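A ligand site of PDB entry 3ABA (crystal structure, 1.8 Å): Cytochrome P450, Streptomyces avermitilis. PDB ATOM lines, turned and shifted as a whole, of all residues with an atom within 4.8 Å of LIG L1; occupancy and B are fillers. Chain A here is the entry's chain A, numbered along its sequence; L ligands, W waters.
SG of Cys 348 binds FE1 of LIG L1 (2.4 Å).
A ring nitrogen (NE2) of His 95 sits at hydrogen-bond distance from an oxygen (O3) of LIG L1 (2.6 Å).
A ring nitrogen (ND1) of His 346 is in hydrogen-bond range of an oxygen (O4) of LIG L1 (2.6 Å).
NH2 of Arg 290 is in salt-bridge range of O1 of LIG L1 (2.7 Å).
The guanidinium group (NH1) of Arg 99 is in salt-bridge range of an oxygen (O3) of LIG L1 (2.8 Å).
The backbone NH (N) of Leu 88 is in hydrogen-bond range of an oxygen (O4) of LIG L1, 3.5 Å away.
The backbone carbonyl oxygen of Leu 87 lies close to an oxygen (O4) of LIG L1.
Residues that only touch LIG L1: Phe 106 (3.3 Å), Ile 151 (3.9 Å), Thr 233 (3.5 Å), Leu 234 (3.7 Å), Ala 237 (3.5 Å), Ala 238 (3.5 Å), Thr 241 (3.0 Å), Thr 242 (3.96 Å), Met 245 (3.8 Å), Leu 278 (3.9 Å), Ile 283 (3.8 Å), Ala 340 (3.4 Å), Phe 341 (3.5 Å), Gly 342 (3.6 Å), Ala 345 (3.6 Å), Ile 349 (3.4 Å), Gly 350 (3.7 Å), Leu 353 (3.99 Å) and Ala 354 (3.7 Å).
Hydrophobic or aromatic side chains within 4 Å of LIG L1: Leu 87, Leu 88, His 95, Phe 106, Ile 151, Leu 234, Ala 237, Ala 238, Met 245, Leu 278, Ile 283, Phe 341, His 346, Ile 349, Leu 353 and Ala 354.
The backbone NH of Cys 348 is in hydrogen-bond range of the backbone carbonyl oxygen of Phe 341 (2.9 Å).
SG of Cys 348 sits close to N of Gly 350.
A ring nitrogen (ND1) of His 346 sits at hydrogen-bond distance from a ring nitrogen (NE2) of His 95, 3.4 Å away.
ND1 of His 346 lies close to O of Leu 87 (3.4 Å).
The guanidinium group (NH1) of Arg 99 lies within hydrogen-bond range of the backbone carbonyl oxygen (O) of Gln 347, at 2.7 Å.
OG1 of Thr 241 is in hydrogen-bond range of O of Ala 237, at 2.7 Å.
O of Ala 238 sits at hydrogen-bond distance from OG1 of Thr 242 (3.0 Å).
The backbone carbonyl oxygen (O) of Gly 342 is in hydrogen-bond range of the side-chain amide nitrogen (NE2) of Gln 347, at 3.0 Å.
Water W1 lies within hydrogen-bond range of an oxygen (O2) of LIG L1 (2.5 Å) and an oxygen (O1) of LG2 L2 (3.1 Å).
Water W2 bridges O1 of LIG L1 and N of Gln 347.
Water W3 lies within hydrogen-bond range of the backbone carbonyl oxygen of Leu 88 and an oxygen (O2) of LIG L1.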
ATOM      1  N   LEU A  87     -16.916  26.199  22.027  1.00  0.00           N
ATOM      2  CA  LEU A  87     -16.158  27.437  22.296  1.00  0.00           C
ATOM      3  C   LEU A  87     -15.068  27.785  21.313  1.00  0.00           C
ATOM      4  O   LEU A  87     -15.065  28.930  20.802  1.00  0.00           O
ATOM      5  CB  LEU A  87     -15.603  27.535  23.743  1.00  0.00           C
ATOM      6  CG  LEU A  87     -16.569  27.355  24.883  1.00  0.00           C
ATOM      7  CD1 LEU A  87     -15.875  27.708  26.198  1.00  0.00           C
ATOM      8  CD2 LEU A  87     -17.897  28.221  24.675  1.00  0.00           C
ATOM      9  N   LEU A  88     -14.120  26.877  21.070  1.00  0.00           N
ATOM     10  CA  LEU A  88     -12.890  27.195  20.307  1.00  0.00           C
ATOM     11  C   LEU A  88     -13.235  27.720  18.908  1.00  0.00           C
ATOM     12  O   LEU A  88     -12.475  28.487  18.338  1.00  0.00           O
ATOM     13  CB  LEU A  88     -12.073  25.936  20.082  1.00  0.00           C
ATOM     14  CG  LEU A  88     -11.277  25.559  21.345  1.00  0.00           C
ATOM     15  CD1 LEU A  88     -10.894  24.081  21.176  1.00  0.00           C
ATOM     16  CD2 LEU A  88      -9.926  26.380  21.468  1.00  0.00           C
ATOM     17  N   HIS A  95     -20.292  32.785  21.191  1.00  0.00           N
ATOM     18  CA  HIS A  95     -19.135  32.362  22.008  1.00  0.00           C
ATOM     19  C   HIS A  95     -19.292  32.947  23.430  1.00  0.00           C
ATOM     20  O   HIS A  95     -19.030  32.253  24.468  1.00  0.00           O
ATOM     21  CB  HIS A  95     -17.841  32.932  21.427  1.00  0.00           C
ATOM     22  CG  HIS A  95     -16.665  32.718  22.316  1.00  0.00           C
ATOM     23  ND1 HIS A  95     -16.127  33.703  23.135  1.00  0.00           N
ATOM     24  CD2 HIS A  95     -15.998  31.567  22.601  1.00  0.00           C
ATOM     25  CE1 HIS A  95     -15.142  33.159  23.844  1.00  0.00           C
ATOM     26  NE2 HIS A  95     -15.050  31.876  23.539  1.00  0.00           N
ATOM     27  N   ARG A  99     -19.834  30.488  26.468  1.00  0.00           N
ATOM     28  CA  ARG A  99     -18.776  30.379  27.451  1.00  0.00           C
ATOM     29  C   ARG A  99     -19.258  30.733  28.886  1.00  0.00           C
ATOM     30  O   ARG A  99     -18.908  30.062  29.890  1.00  0.00           O
ATOM     31  CB  ARG A  99     -17.590  31.263  27.066  1.00  0.00           C
ATOM     32  CG  ARG A  99     -16.479  31.163  28.097  1.00  0.00           C
ATOM     33  CD  ARG A  99     -15.151  31.550  27.539  1.00  0.00           C
ATOM     34  NE  ARG A  99     -14.172  31.649  28.629  1.00  0.00           N
ATOM     35  CZ  ARG A  99     -12.854  31.479  28.471  1.00  0.00           C
ATOM     36  NH1 ARG A  99     -12.352  31.159  27.268  1.00  0.00           N
ATOM     37  NH2 ARG A  99     -12.008  31.682  29.537  1.00  0.00           N
ATOM     38  N   PHE A 106     -18.477  25.196  35.409  1.00  0.00           N
ATOM     39  CA  PHE A 106     -17.064  24.758  35.464  1.00  0.00           C
ATOM     40  C   PHE A 106     -16.321  25.957  36.036  1.00  0.00           C
ATOM     41  O   PHE A 106     -15.842  26.833  35.298  1.00  0.00           O
ATOM     42  CB  PHE A 106     -16.582  24.452  34.044  1.00  0.00           C
ATOM     43  CG  PHE A 106     -15.125  23.964  33.935  1.00  0.00           C
ATOM     44  CD1 PHE A 106     -14.625  22.930  34.780  1.00  0.00           C
ATOM     45  CD2 PHE A 106     -14.298  24.495  32.980  1.00  0.00           C
ATOM     46  CE1 PHE A 106     -13.300  22.522  34.668  1.00  0.00           C
ATOM     47  CE2 PHE A 106     -12.954  24.122  32.875  1.00  0.00           C
ATOM     48  CZ  PHE A 106     -12.455  23.122  33.697  1.00  0.00           C
ATOM     49  N   ILE A 151      -9.723  14.420  34.416  1.00  0.00           N
ATOM     50  CA  ILE A 151     -10.858  14.989  33.703  1.00  0.00           C
ATOM     51  C   ILE A 151     -11.996  13.959  33.543  1.00  0.00           C
ATOM     52  O   ILE A 151     -13.165  14.297  33.536  1.00  0.00           O
ATOM     53  CB  ILE A 151     -10.382  15.613  32.343  1.00  0.00           C
ATOM     54  CG1 ILE A 151     -11.527  16.548  31.815  1.00  0.00           C
ATOM     55  CG2 ILE A 151     -10.120  14.535  31.250  1.00  0.00           C
ATOM     56  CD1 ILE A 151     -11.633  17.832  32.697  1.00  0.00           C
ATOM     57  N   THR A 233     -14.800  19.173  23.790  1.00  0.00           N
ATOM     58  CA  THR A 233     -13.736  20.145  23.857  1.00  0.00           C
ATOM     59  C   THR A 233     -13.012  20.050  25.199  1.00  0.00           C
ATOM     60  O   THR A 233     -11.777  19.932  25.218  1.00  0.00           O
ATOM     61  CB  THR A 233     -14.204  21.562  23.669  1.00  0.00           C
ATOM     62  OG1 THR A 233     -14.696  21.609  22.346  1.00  0.00           O
ATOM     63  CG2 THR A 233     -13.002  22.525  23.670  1.00  0.00           C
ATOM     64  N   LEU A 234     -13.792  20.013  26.300  1.00  0.00           N
ATOM     65  CA  LEU A 234     -13.150  19.943  27.604  1.00  0.00           C
ATOM     66  C   LEU A 234     -12.385  18.649  27.778  1.00  0.00           C
ATOM     67  O   LEU A 234     -11.238  18.651  28.331  1.00  0.00           O
ATOM     68  CB  LEU A 234     -14.164  20.078  28.703  1.00  0.00           C
ATOM     69  CG  LEU A 234     -14.786  21.505  28.644  1.00  0.00           C
ATOM     70  CD1 LEU A 234     -16.119  21.389  29.443  1.00  0.00           C
ATOM     71  CD2 LEU A 234     -13.835  22.453  29.291  1.00  0.00           C
ATOM     72  N   ALA A 237      -9.171  18.604  25.345  1.00  0.00           N
ATOM     73  CA  ALA A 237      -8.177  19.639  25.648  1.00  0.00           C
ATOM     74  C   ALA A 237      -7.487  19.188  26.953  1.00  0.00           C
ATOM     75  O   ALA A 237      -6.270  19.222  27.097  1.00  0.00           O
ATOM     76  CB  ALA A 237      -8.913  21.044  25.944  1.00  0.00           C
ATOM     77  N   ALA A 238      -8.285  18.753  27.935  1.00  0.00           N
ATOM     78  CA  ALA A 238      -7.708  18.465  29.259  1.00  0.00           C
ATOM     79  C   ALA A 238      -6.822  17.243  29.242  1.00  0.00           C
ATOM     80  O   ALA A 238      -5.883  17.212  30.072  1.00  0.00           O
ATOM     81  CB  ALA A 238      -8.865  18.286  30.362  1.00  0.00           C
ATOM     82  N   THR A 241      -3.248  18.432  26.272  1.00  0.00           N
ATOM     83  CA  THR A 241      -2.305  19.519  26.579  1.00  0.00           C
ATOM     84  C   THR A 241      -1.568  19.157  27.860  1.00  0.00           C
ATOM     85  O   THR A 241      -0.314  19.205  27.922  1.00  0.00           O
ATOM     86  CB  THR A 241      -3.033  20.858  26.782  1.00  0.00           C
ATOM     87  OG1 THR A 241      -4.067  20.691  27.759  1.00  0.00           O
ATOM     88  CG2 THR A 241      -3.729  21.293  25.547  1.00  0.00           C
ATOM     89  N   THR A 242      -2.323  18.754  28.893  1.00  0.00           N
ATOM     90  CA  THR A 242      -1.688  18.526  30.202  1.00  0.00           C
ATOM     91  C   THR A 242      -0.727  17.316  30.093  1.00  0.00           C
ATOM     92  O   THR A 242       0.375  17.374  30.573  1.00  0.00           O
ATOM     93  CB  THR A 242      -2.816  18.159  31.225  1.00  0.00           C
ATOM     94  OG1 THR A 242      -3.863  19.157  31.086  1.00  0.00           O
ATOM     95  CG2 THR A 242      -2.233  18.240  32.625  1.00  0.00           C
ATOM     96  N   MET A 245       2.437  18.588  28.485  1.00  0.00           N
ATOM     97  CA  MET A 245       3.275  19.410  29.439  1.00  0.00           C
ATOM     98  C   MET A 245       4.012  18.508  30.472  1.00  0.00           C
ATOM     99  O   MET A 245       5.096  18.820  30.891  1.00  0.00           O
ATOM    100  CB  MET A 245       2.389  20.448  30.229  1.00  0.00           C
ATOM    101  CG  MET A 245       2.204  21.807  29.421  1.00  0.00           C
ATOM    102  SD  MET A 245       3.761  22.567  28.983  1.00  0.00           S
ATOM    103  CE  MET A 245       4.451  22.929  30.669  1.00  0.00           C
ATOM    104  N   LEU A 278       5.515  26.523  31.449  1.00  0.00           N
ATOM    105  CA  LEU A 278       4.473  26.857  30.468  1.00  0.00           C
ATOM    106  C   LEU A 278       5.059  27.818  29.490  1.00  0.00           C
ATOM    107  O   LEU A 278       4.898  27.623  28.288  1.00  0.00           O
ATOM    108  CB  LEU A 278       3.238  27.526  31.131  1.00  0.00           C
ATOM    109  CG  LEU A 278       2.504  26.392  31.890  1.00  0.00           C
ATOM    110  CD1 LEU A 278       1.532  26.913  32.961  1.00  0.00           C
ATOM    111  CD2 LEU A 278       1.557  25.568  30.941  1.00  0.00           C
ATOM    112  N   ILE A 283       3.495  24.730  24.335  1.00  0.00           N
ATOM    113  CA  ILE A 283       3.334  23.489  23.564  1.00  0.00           C
ATOM    114  C   ILE A 283       2.454  23.667  22.347  1.00  0.00           C
ATOM    115  O   ILE A 283       2.499  22.798  21.408  1.00  0.00           O
ATOM    116  CB  ILE A 283       2.788  22.313  24.449  1.00  0.00           C
ATOM    117  CG1 ILE A 283       1.614  22.799  25.274  1.00  0.00           C
ATOM    118  CG2 ILE A 283       3.923  21.765  25.389  1.00  0.00           C
ATOM    119  CD1 ILE A 283       0.651  21.663  25.819  1.00  0.00           C
ATOM    120  N   GLY A 288      -2.129  29.822  17.041  1.00  0.00           N
ATOM    121  CA  GLY A 288      -3.560  29.857  16.848  1.00  0.00           C
ATOM    122  C   GLY A 288      -3.925  30.485  15.497  1.00  0.00           C
ATOM    123  O   GLY A 288      -3.233  31.370  15.024  1.00  0.00           O
ATOM    124  N   ARG A 290      -6.515  32.679  13.039  1.00  0.00           N
ATOM    125  CA  ARG A 290      -7.674  33.582  13.058  1.00  0.00           C
ATOM    126  C   ARG A 290      -7.851  34.180  11.636  1.00  0.00           C
ATOM    127  O   ARG A 290      -6.966  34.061  10.792  1.00  0.00           O
ATOM    128  CB  ARG A 290      -7.406  34.786  13.977  1.00  0.00           C
ATOM    129  CG  ARG A 290      -7.230  34.509  15.515  1.00  0.00           C
ATOM    130  CD  ARG A 290      -8.504  33.881  16.053  1.00  0.00           C
ATOM    131  NE  ARG A 290      -8.455  33.798  17.523  1.00  0.00           N
ATOM    132  CZ  ARG A 290      -8.031  32.742  18.230  1.00  0.00           C
ATOM    133  NH1 ARG A 290      -7.644  31.567  17.638  1.00  0.00           N
ATOM    134  NH2 ARG A 290      -8.042  32.818  19.558  1.00  0.00           N
ATOM    135  N   ALA A 340       0.953  30.809  26.858  1.00  0.00           N
ATOM    136  CA  ALA A 340       0.804  29.331  26.656  1.00  0.00           C
ATOM    137  C   ALA A 340      -0.682  28.943  26.622  1.00  0.00           C
ATOM    138  O   ALA A 340      -1.050  27.933  26.008  1.00  0.00           O
ATOM    139  CB  ALA A 340       1.601  28.556  27.768  1.00  0.00           C
ATOM    140  N   PHE A 341      -1.546  29.716  27.328  1.00  0.00           N
ATOM    141  CA  PHE A 341      -3.013  29.479  27.323  1.00  0.00           C
ATOM    142  C   PHE A 341      -3.726  30.445  26.404  1.00  0.00           C
ATOM    143  O   PHE A 341      -4.945  30.616  26.526  1.00  0.00           O
ATOM    144  CB  PHE A 341      -3.554  29.697  28.746  1.00  0.00           C
ATOM    145  CG  PHE A 341      -2.996  28.683  29.753  1.00  0.00           C
ATOM    146  CD1 PHE A 341      -3.374  27.313  29.637  1.00  0.00           C
ATOM    147  CD2 PHE A 341      -2.186  29.106  30.814  1.00  0.00           C
ATOM    148  CE1 PHE A 341      -2.951  26.360  30.594  1.00  0.00           C
ATOM    149  CE2 PHE A 341      -1.732  28.154  31.770  1.00  0.00           C
ATOM    150  CZ  PHE A 341      -2.110  26.784  31.653  1.00  0.00           C
ATOM    151  N   GLY A 342      -2.957  31.128  25.576  1.00  0.00           N
ATOM    152  CA  GLY A 342      -3.648  32.115  24.680  1.00  0.00           C
ATOM    153  C   GLY A 342      -3.952  33.408  25.407  1.00  0.00           C
ATOM    154  O   GLY A 342      -3.341  33.720  26.420  1.00  0.00           O
ATOM    155  N   ALA A 345     -10.582  36.682  24.197  1.00  0.00           N
ATOM    156  CA  ALA A 345     -11.827  35.996  24.457  1.00  0.00           C
ATOM    157  C   ALA A 345     -11.691  34.461  24.563  1.00  0.00           C
ATOM    158  O   ALA A 345     -12.487  33.844  25.282  1.00  0.00           O
ATOM    159  CB  ALA A 345     -12.905  36.361  23.391  1.00  0.00           C
ATOM    160  N   HIS A 346     -10.763  33.883  23.803  1.00  0.00           N
ATOM    161  CA  HIS A 346     -10.605  32.423  23.764  1.00  0.00           C
ATOM    162  C   HIS A 346      -9.607  31.867  24.754  1.00  0.00           C
ATOM    163  O   HIS A 346      -9.343  30.661  24.755  1.00  0.00           O
ATOM    164  CB  HIS A 346     -10.321  31.894  22.305  1.00  0.00           C
ATOM    165  CG  HIS A 346     -11.516  32.050  21.407  1.00  0.00           C
ATOM    166  ND1 HIS A 346     -12.560  31.163  21.392  1.00  0.00           N
ATOM    167  CD2 HIS A 346     -11.856  33.039  20.540  1.00  0.00           C
ATOM    168  CE1 HIS A 346     -13.459  31.525  20.502  1.00  0.00           C
ATOM    169  NE2 HIS A 346     -13.056  32.665  19.967  1.00  0.00           N
ATOM    170  N   GLN A 347      -9.007  32.746  25.568  1.00  0.00           N
ATOM    171  CA  GLN A 347      -8.013  32.257  26.513  1.00  0.00           C
ATOM    172  C   GLN A 347      -8.542  31.070  27.337  1.00  0.00           C
ATOM    173  O   GLN A 347      -9.680  31.078  27.847  1.00  0.00           O
ATOM    174  CB  GLN A 347      -7.523  33.391  27.450  1.00  0.00           C
ATOM    175  CG  GLN A 347      -6.399  32.886  28.363  1.00  0.00           C
ATOM    176  CD  GLN A 347      -5.797  33.981  29.331  1.00  0.00           C
ATOM    177  OE1 GLN A 347      -6.397  34.287  30.361  1.00  0.00           O
ATOM    178  NE2 GLN A 347      -4.674  34.560  28.967  1.00  0.00           N
ATOM    179  N   CYS A 348      -7.654  30.092  27.486  1.00  0.00           N
ATOM    180  CA  CYS A 348      -7.991  28.771  28.075  1.00  0.00           C
ATOM    181  C   CYS A 348      -8.969  28.834  29.263  1.00  0.00           C
ATOM    182  O   CYS A 348      -8.655  29.466  30.276  1.00  0.00           O
ATOM    183  CB  CYS A 348      -6.674  28.084  28.536  1.00  0.00           C
ATOM    184  SG  CYS A 348      -7.091  26.417  29.204  1.00  0.00           S
ATOM    185  N   ILE A 349     -10.163  28.254  29.172  1.00  0.00           N
ATOM    186  CA  ILE A 349     -11.064  28.284  30.295  1.00  0.00           C
ATOM    187  C   ILE A 349     -10.592  27.287  31.416  1.00  0.00           C
ATOM    188  O   ILE A 349     -11.031  27.392  32.579  1.00  0.00           O
ATOM    189  CB  ILE A 349     -12.499  27.908  29.827  1.00  0.00           C
ATOM    190  CG1 ILE A 349     -13.548  28.250  30.914  1.00  0.00           C
ATOM    191  CG2 ILE A 349     -12.551  26.481  29.378  1.00  0.00           C
ATOM    192  CD1 ILE A 349     -14.993  28.111  30.338  1.00  0.00           C
ATOM    193  N   GLY A 350      -9.719  26.395  31.052  1.00  0.00           N
ATOM    194  CA  GLY A 350      -9.285  25.308  31.963  1.00  0.00           C
ATOM    195  C   GLY A 350      -7.929  25.574  32.603  1.00  0.00           C
ATOM    196  O   GLY A 350      -7.379  24.675  33.289  1.00  0.00           O
ATOM    197  N   LEU A 353      -7.240  24.652  36.325  1.00  0.00           N
ATOM    198  CA  LEU A 353      -7.162  23.207  36.506  1.00  0.00           C
ATOM    199  C   LEU A 353      -5.815  22.651  35.936  1.00  0.00           C
ATOM    200  O   LEU A 353      -5.209  21.815  36.555  1.00  0.00           O
ATOM    201  CB  LEU A 353      -8.388  22.479  35.874  1.00  0.00           C
ATOM    202  CG  LEU A 353      -8.265  20.917  35.906  1.00  0.00           C
ATOM    203  CD1 LEU A 353      -8.197  20.394  37.368  1.00  0.00           C
ATOM    204  CD2 LEU A 353      -9.481  20.237  35.287  1.00  0.00           C
ATOM    205  N   ALA A 354      -5.388  23.093  34.752  1.00  0.00           N
ATOM    206  CA  ALA A 354      -4.105  22.709  34.162  1.00  0.00           C
ATOM    207  C   ALA A 354      -2.975  23.045  35.158  1.00  0.00           C
ATOM    208  O   ALA A 354      -2.085  22.203  35.416  1.00  0.00           O
ATOM    209  CB  ALA A 354      -3.932  23.517  32.841  1.00  0.00           C
ATOM    210  N   GLU A 357      -3.039  20.731  38.220  1.00  0.00           N
ATOM    211  CA  GLU A 357      -2.535  19.344  37.884  1.00  0.00           C
ATOM    212  C   GLU A 357      -1.039  19.383  37.780  1.00  0.00           C
ATOM    213  O   GLU A 357      -0.346  18.520  38.320  1.00  0.00           O
ATOM    214  CB  GLU A 357      -3.175  18.812  36.569  1.00  0.00           C
ATOM    215  CG  GLU A 357      -4.673  18.500  36.742  1.00  0.00           C
ATOM    216  CD  GLU A 357      -5.175  17.704  35.477  1.00  0.00           C
ATOM    217  OE1 GLU A 357      -4.526  16.664  35.198  1.00  0.00           O
ATOM    218  OE2 GLU A 357      -6.153  18.104  34.842  1.00  0.00           O
ATOM    219  N   LEU A 358      -0.511  20.387  37.067  1.00  0.00           N
ATOM    220  CA  LEU A 358       0.961  20.418  36.860  1.00  0.00           C
ATOM    221  C   LEU A 358       1.727  20.611  38.168  1.00  0.00           C
ATOM    222  O   LEU A 358       2.800  19.999  38.366  1.00  0.00           O
ATOM    223  CB  LEU A 358       1.402  21.483  35.828  1.00  0.00           C
ATOM    224  CG  LEU A 358       0.836  21.066  34.414  1.00  0.00           C
ATOM    225  CD1 LEU A 358       1.268  22.265  33.461  1.00  0.00           C
ATOM    226  CD2 LEU A 358       1.449  19.678  33.861  1.00  0.00           C
HETATM  227  C1  LIG L   1      -8.447  27.113  25.026  1.00  0.00           C
HETATM  228  C2  LIG L   1      -3.876  25.884  25.917  1.00  0.00           C
HETATM  229  C3  LIG L   1      -5.517  22.808  29.386  1.00  0.00           C
HETATM  230  C4  LIG L   1     -10.091  23.619  28.031  1.00  0.00           C
HETATM  231  C5  LIG L   1      -7.104  27.099  25.054  1.00  0.00           C
HETATM  232  C6  LIG L   1      -6.259  27.918  24.184  1.00  0.00           C
HETATM  233  C7  LIG L   1      -4.969  27.581  24.441  1.00  0.00           C
HETATM  234  C8  LIG L   1      -4.993  26.533  25.419  1.00  0.00           C
HETATM  235  C9  LIG L   1      -3.687  28.062  23.797  1.00  0.00           C
HETATM  236  C10 LIG L   1      -6.746  29.027  23.224  1.00  0.00           C
HETATM  237  C11 LIG L   1      -6.773  28.509  21.742  1.00  0.00           C
HETATM  238  C12 LIG L   1      -7.051  29.690  20.780  1.00  0.00           C
HETATM  239  O1  LIG L   1      -7.037  30.865  21.186  1.00  0.00           O
HETATM  240  O2  LIG L   1      -7.322  29.457  19.574  1.00  0.00           O
HETATM  241  C13 LIG L   1      -3.930  24.965  26.954  1.00  0.00           C
HETATM  242  C14 LIG L   1      -2.757  24.363  27.603  1.00  0.00           C
HETATM  243  C15 LIG L   1      -3.238  23.568  28.558  1.00  0.00           C
HETATM  244  C16 LIG L   1      -4.681  23.554  28.522  1.00  0.00           C
HETATM  245  C17 LIG L   1      -1.244  24.656  27.319  1.00  0.00           C
HETATM  246  C18 LIG L   1      -2.454  22.677  29.531  1.00  0.00           C
HETATM  247  C19 LIG L   1      -1.333  23.035  30.124  1.00  0.00           C
HETATM  248  C20 LIG L   1      -6.888  22.795  29.401  1.00  0.00           C
HETATM  249  C21 LIG L   1      -7.722  22.031  30.304  1.00  0.00           C
HETATM  250  C22 LIG L   1      -8.938  22.288  29.881  1.00  0.00           C
HETATM  251  C23 LIG L   1      -8.957  23.136  28.744  1.00  0.00           C
HETATM  252  C24 LIG L   1      -7.238  21.174  31.543  1.00  0.00           C
HETATM  253  C25 LIG L   1     -10.277  21.804  30.379  1.00  0.00           C
HETATM  254  C26 LIG L   1     -10.543  21.447  31.632  1.00  0.00           C
HETATM  255  C27 LIG L   1     -10.007  24.581  27.019  1.00  0.00           C
HETATM  256  C28 LIG L   1     -11.200  25.102  26.327  1.00  0.00           C
HETATM  257  C29 LIG L   1     -10.693  26.185  25.424  1.00  0.00           C
HETATM  258  C30 LIG L   1      -9.294  26.218  25.604  1.00  0.00           C
HETATM  259  C31 LIG L   1     -12.633  24.590  26.529  1.00  0.00           C
HETATM  260  C32 LIG L   1     -11.564  27.046  24.497  1.00  0.00           C
HETATM  261  C33 LIG L   1     -11.934  28.331  25.293  1.00  0.00           C
HETATM  262  C34 LIG L   1     -12.668  29.366  24.360  1.00  0.00           C
HETATM  263  O3  LIG L   1     -13.328  30.354  24.818  1.00  0.00           O
HETATM  264  O4  LIG L   1     -12.570  29.172  23.136  1.00  0.00           O
HETATM  265  N1  LIG L   1      -6.273  26.200  25.741  1.00  0.00           N
HETATM  266  N2  LIG L   1      -5.066  24.430  27.496  1.00  0.00           N
HETATM  267  N3  LIG L   1      -7.676  23.442  28.432  1.00  0.00           N
HETATM  268  N4  LIG L   1      -8.942  25.272  26.530  1.00  0.00           N
HETATM  269 FE1  LIG L   1      -6.982  24.993  27.221  1.00  0.00          FE
HETATM  270  C1  LG2 L   2      -6.635  23.588  19.734  1.00  0.00           C
HETATM  271  O1  LG2 L   2      -7.539  24.431  19.594  1.00  0.00           O
HETATM  272  C2  LG2 L   2      -5.759  23.159  18.546  1.00  0.00           C
HETATM  273  C3  LG2 L   2      -6.613  22.614  17.362  1.00  0.00           C
HETATM  274  C4  LG2 L   2      -7.581  21.446  17.791  1.00  0.00           C
HETATM  275  C5  LG2 L   2      -8.368  20.907  16.558  1.00  0.00           C
HETATM  276  C6  LG2 L   2      -9.284  19.740  17.016  1.00  0.00           C
HETATM  277  C7  LG2 L   2     -10.100  19.217  15.801  1.00  0.00           C
HETATM  278  C8  LG2 L   2     -11.371  18.506  16.370  1.00  0.00           C
HETATM  279  C9  LG2 L   2     -12.266  18.017  15.198  1.00  0.00           C
HETATM  280  C10 LG2 L   2     -13.495  17.237  15.780  1.00  0.00           C
HETATM  281  C11 LG2 L   2     -14.514  16.916  14.583  1.00  0.00           C
HETATM  282  C12 LG2 L   2     -15.767  16.156  15.105  1.00  0.00           C
HETATM  283  C13 LG2 L   2     -16.823  17.132  15.658  1.00  0.00           C
HETATM  284  C14 LG2 L   2     -17.975  16.352  16.376  1.00  0.00           C
HETATM  285  C15 LG2 L   2     -17.649  15.471  17.652  1.00  0.00           C
HETATM  286  C16 LG2 L   2     -17.000  16.421  18.683  1.00  0.00           C
HETATM  287  C17 LG2 L   2     -15.608  16.526  18.741  1.00  0.00           C
HETATM  288  C18 LG2 L   2     -14.953  17.528  19.507  1.00  0.00           C
HETATM  289  C19 LG2 L   2     -13.568  17.602  19.597  1.00  0.00           C
HETATM  290  C20 LG2 L   2      -4.921  24.376  18.147  1.00  0.00           C
HETATM  291  C21 LG2 L   2     -12.873  18.579  20.350  1.00  0.00           C
HETATM  292  C22 LG2 L   2     -11.449  18.596  20.396  1.00  0.00           C
HETATM  293  C23 LG2 L   2     -10.818  19.646  21.092  1.00  0.00           C
HETATM  294  C24 LG2 L   2      -9.459  19.777  21.311  1.00  0.00           C
HETATM  295  C25 LG2 L   2      -9.034  20.874  22.126  1.00  0.00           C
HETATM  296  C26 LG2 L   2      -7.662  21.161  22.244  1.00  0.00           C
HETATM  297  C27 LG2 L   2      -7.187  22.258  23.057  1.00  0.00           C
HETATM  298  C28 LG2 L   2      -7.254  23.492  22.131  1.00  0.00           C
HETATM  299  C29 LG2 L   2      -6.552  24.726  22.713  1.00  0.00           C
HETATM  300  C30 LG2 L   2     -17.973  17.361  19.503  1.00  0.00           C
HETATM  301  C31 LG2 L   2      -4.119  25.051  19.339  1.00  0.00           C
HETATM  302  O2  LG2 L   2      -6.387  23.077  20.982  1.00  0.00           O
HETATM  303  C32 LG2 L   2      -3.311  26.261  18.954  1.00  0.00           C
HETATM  304  C33 LG2 L   2      -2.612  26.759  20.227  1.00  0.00           C
HETATM  305  C34 LG2 L   2      -1.772  28.052  20.120  1.00  0.00           C
HETATM  306  C35 LG2 L   2      -2.652  29.301  20.468  1.00  0.00           C
HETATM  307  O3  LG2 L   2      -5.647  22.128  16.385  1.00  0.00           O
HETATM  308  O4  LG2 L   2      -7.399  20.339  15.590  1.00  0.00           O
HETATM  309  O5  LG2 L   2      -9.262  18.246  15.084  1.00  0.00           O
HETATM  310  O6  LG2 L   2     -11.451  17.114  14.435  1.00  0.00           O
HETATM  311  O7  LG2 L   2     -13.861  16.065  13.604  1.00  0.00           O
HETATM  312  O8  LG2 L   2     -17.279  18.021  14.619  1.00  0.00           O
HETATM  313  O9  LG2 L   2     -18.994  14.992  18.021  1.00  0.00           O
HETATM  314  O   HOH W   1      -7.017  27.230  18.458  1.00  0.00           O
HETATM  315  O   HOH W   2      -6.694  32.747  22.949  1.00  0.00           O
HETATM  316  O   HOH W   3      -9.715  28.290  17.527  1.00  0.00           O
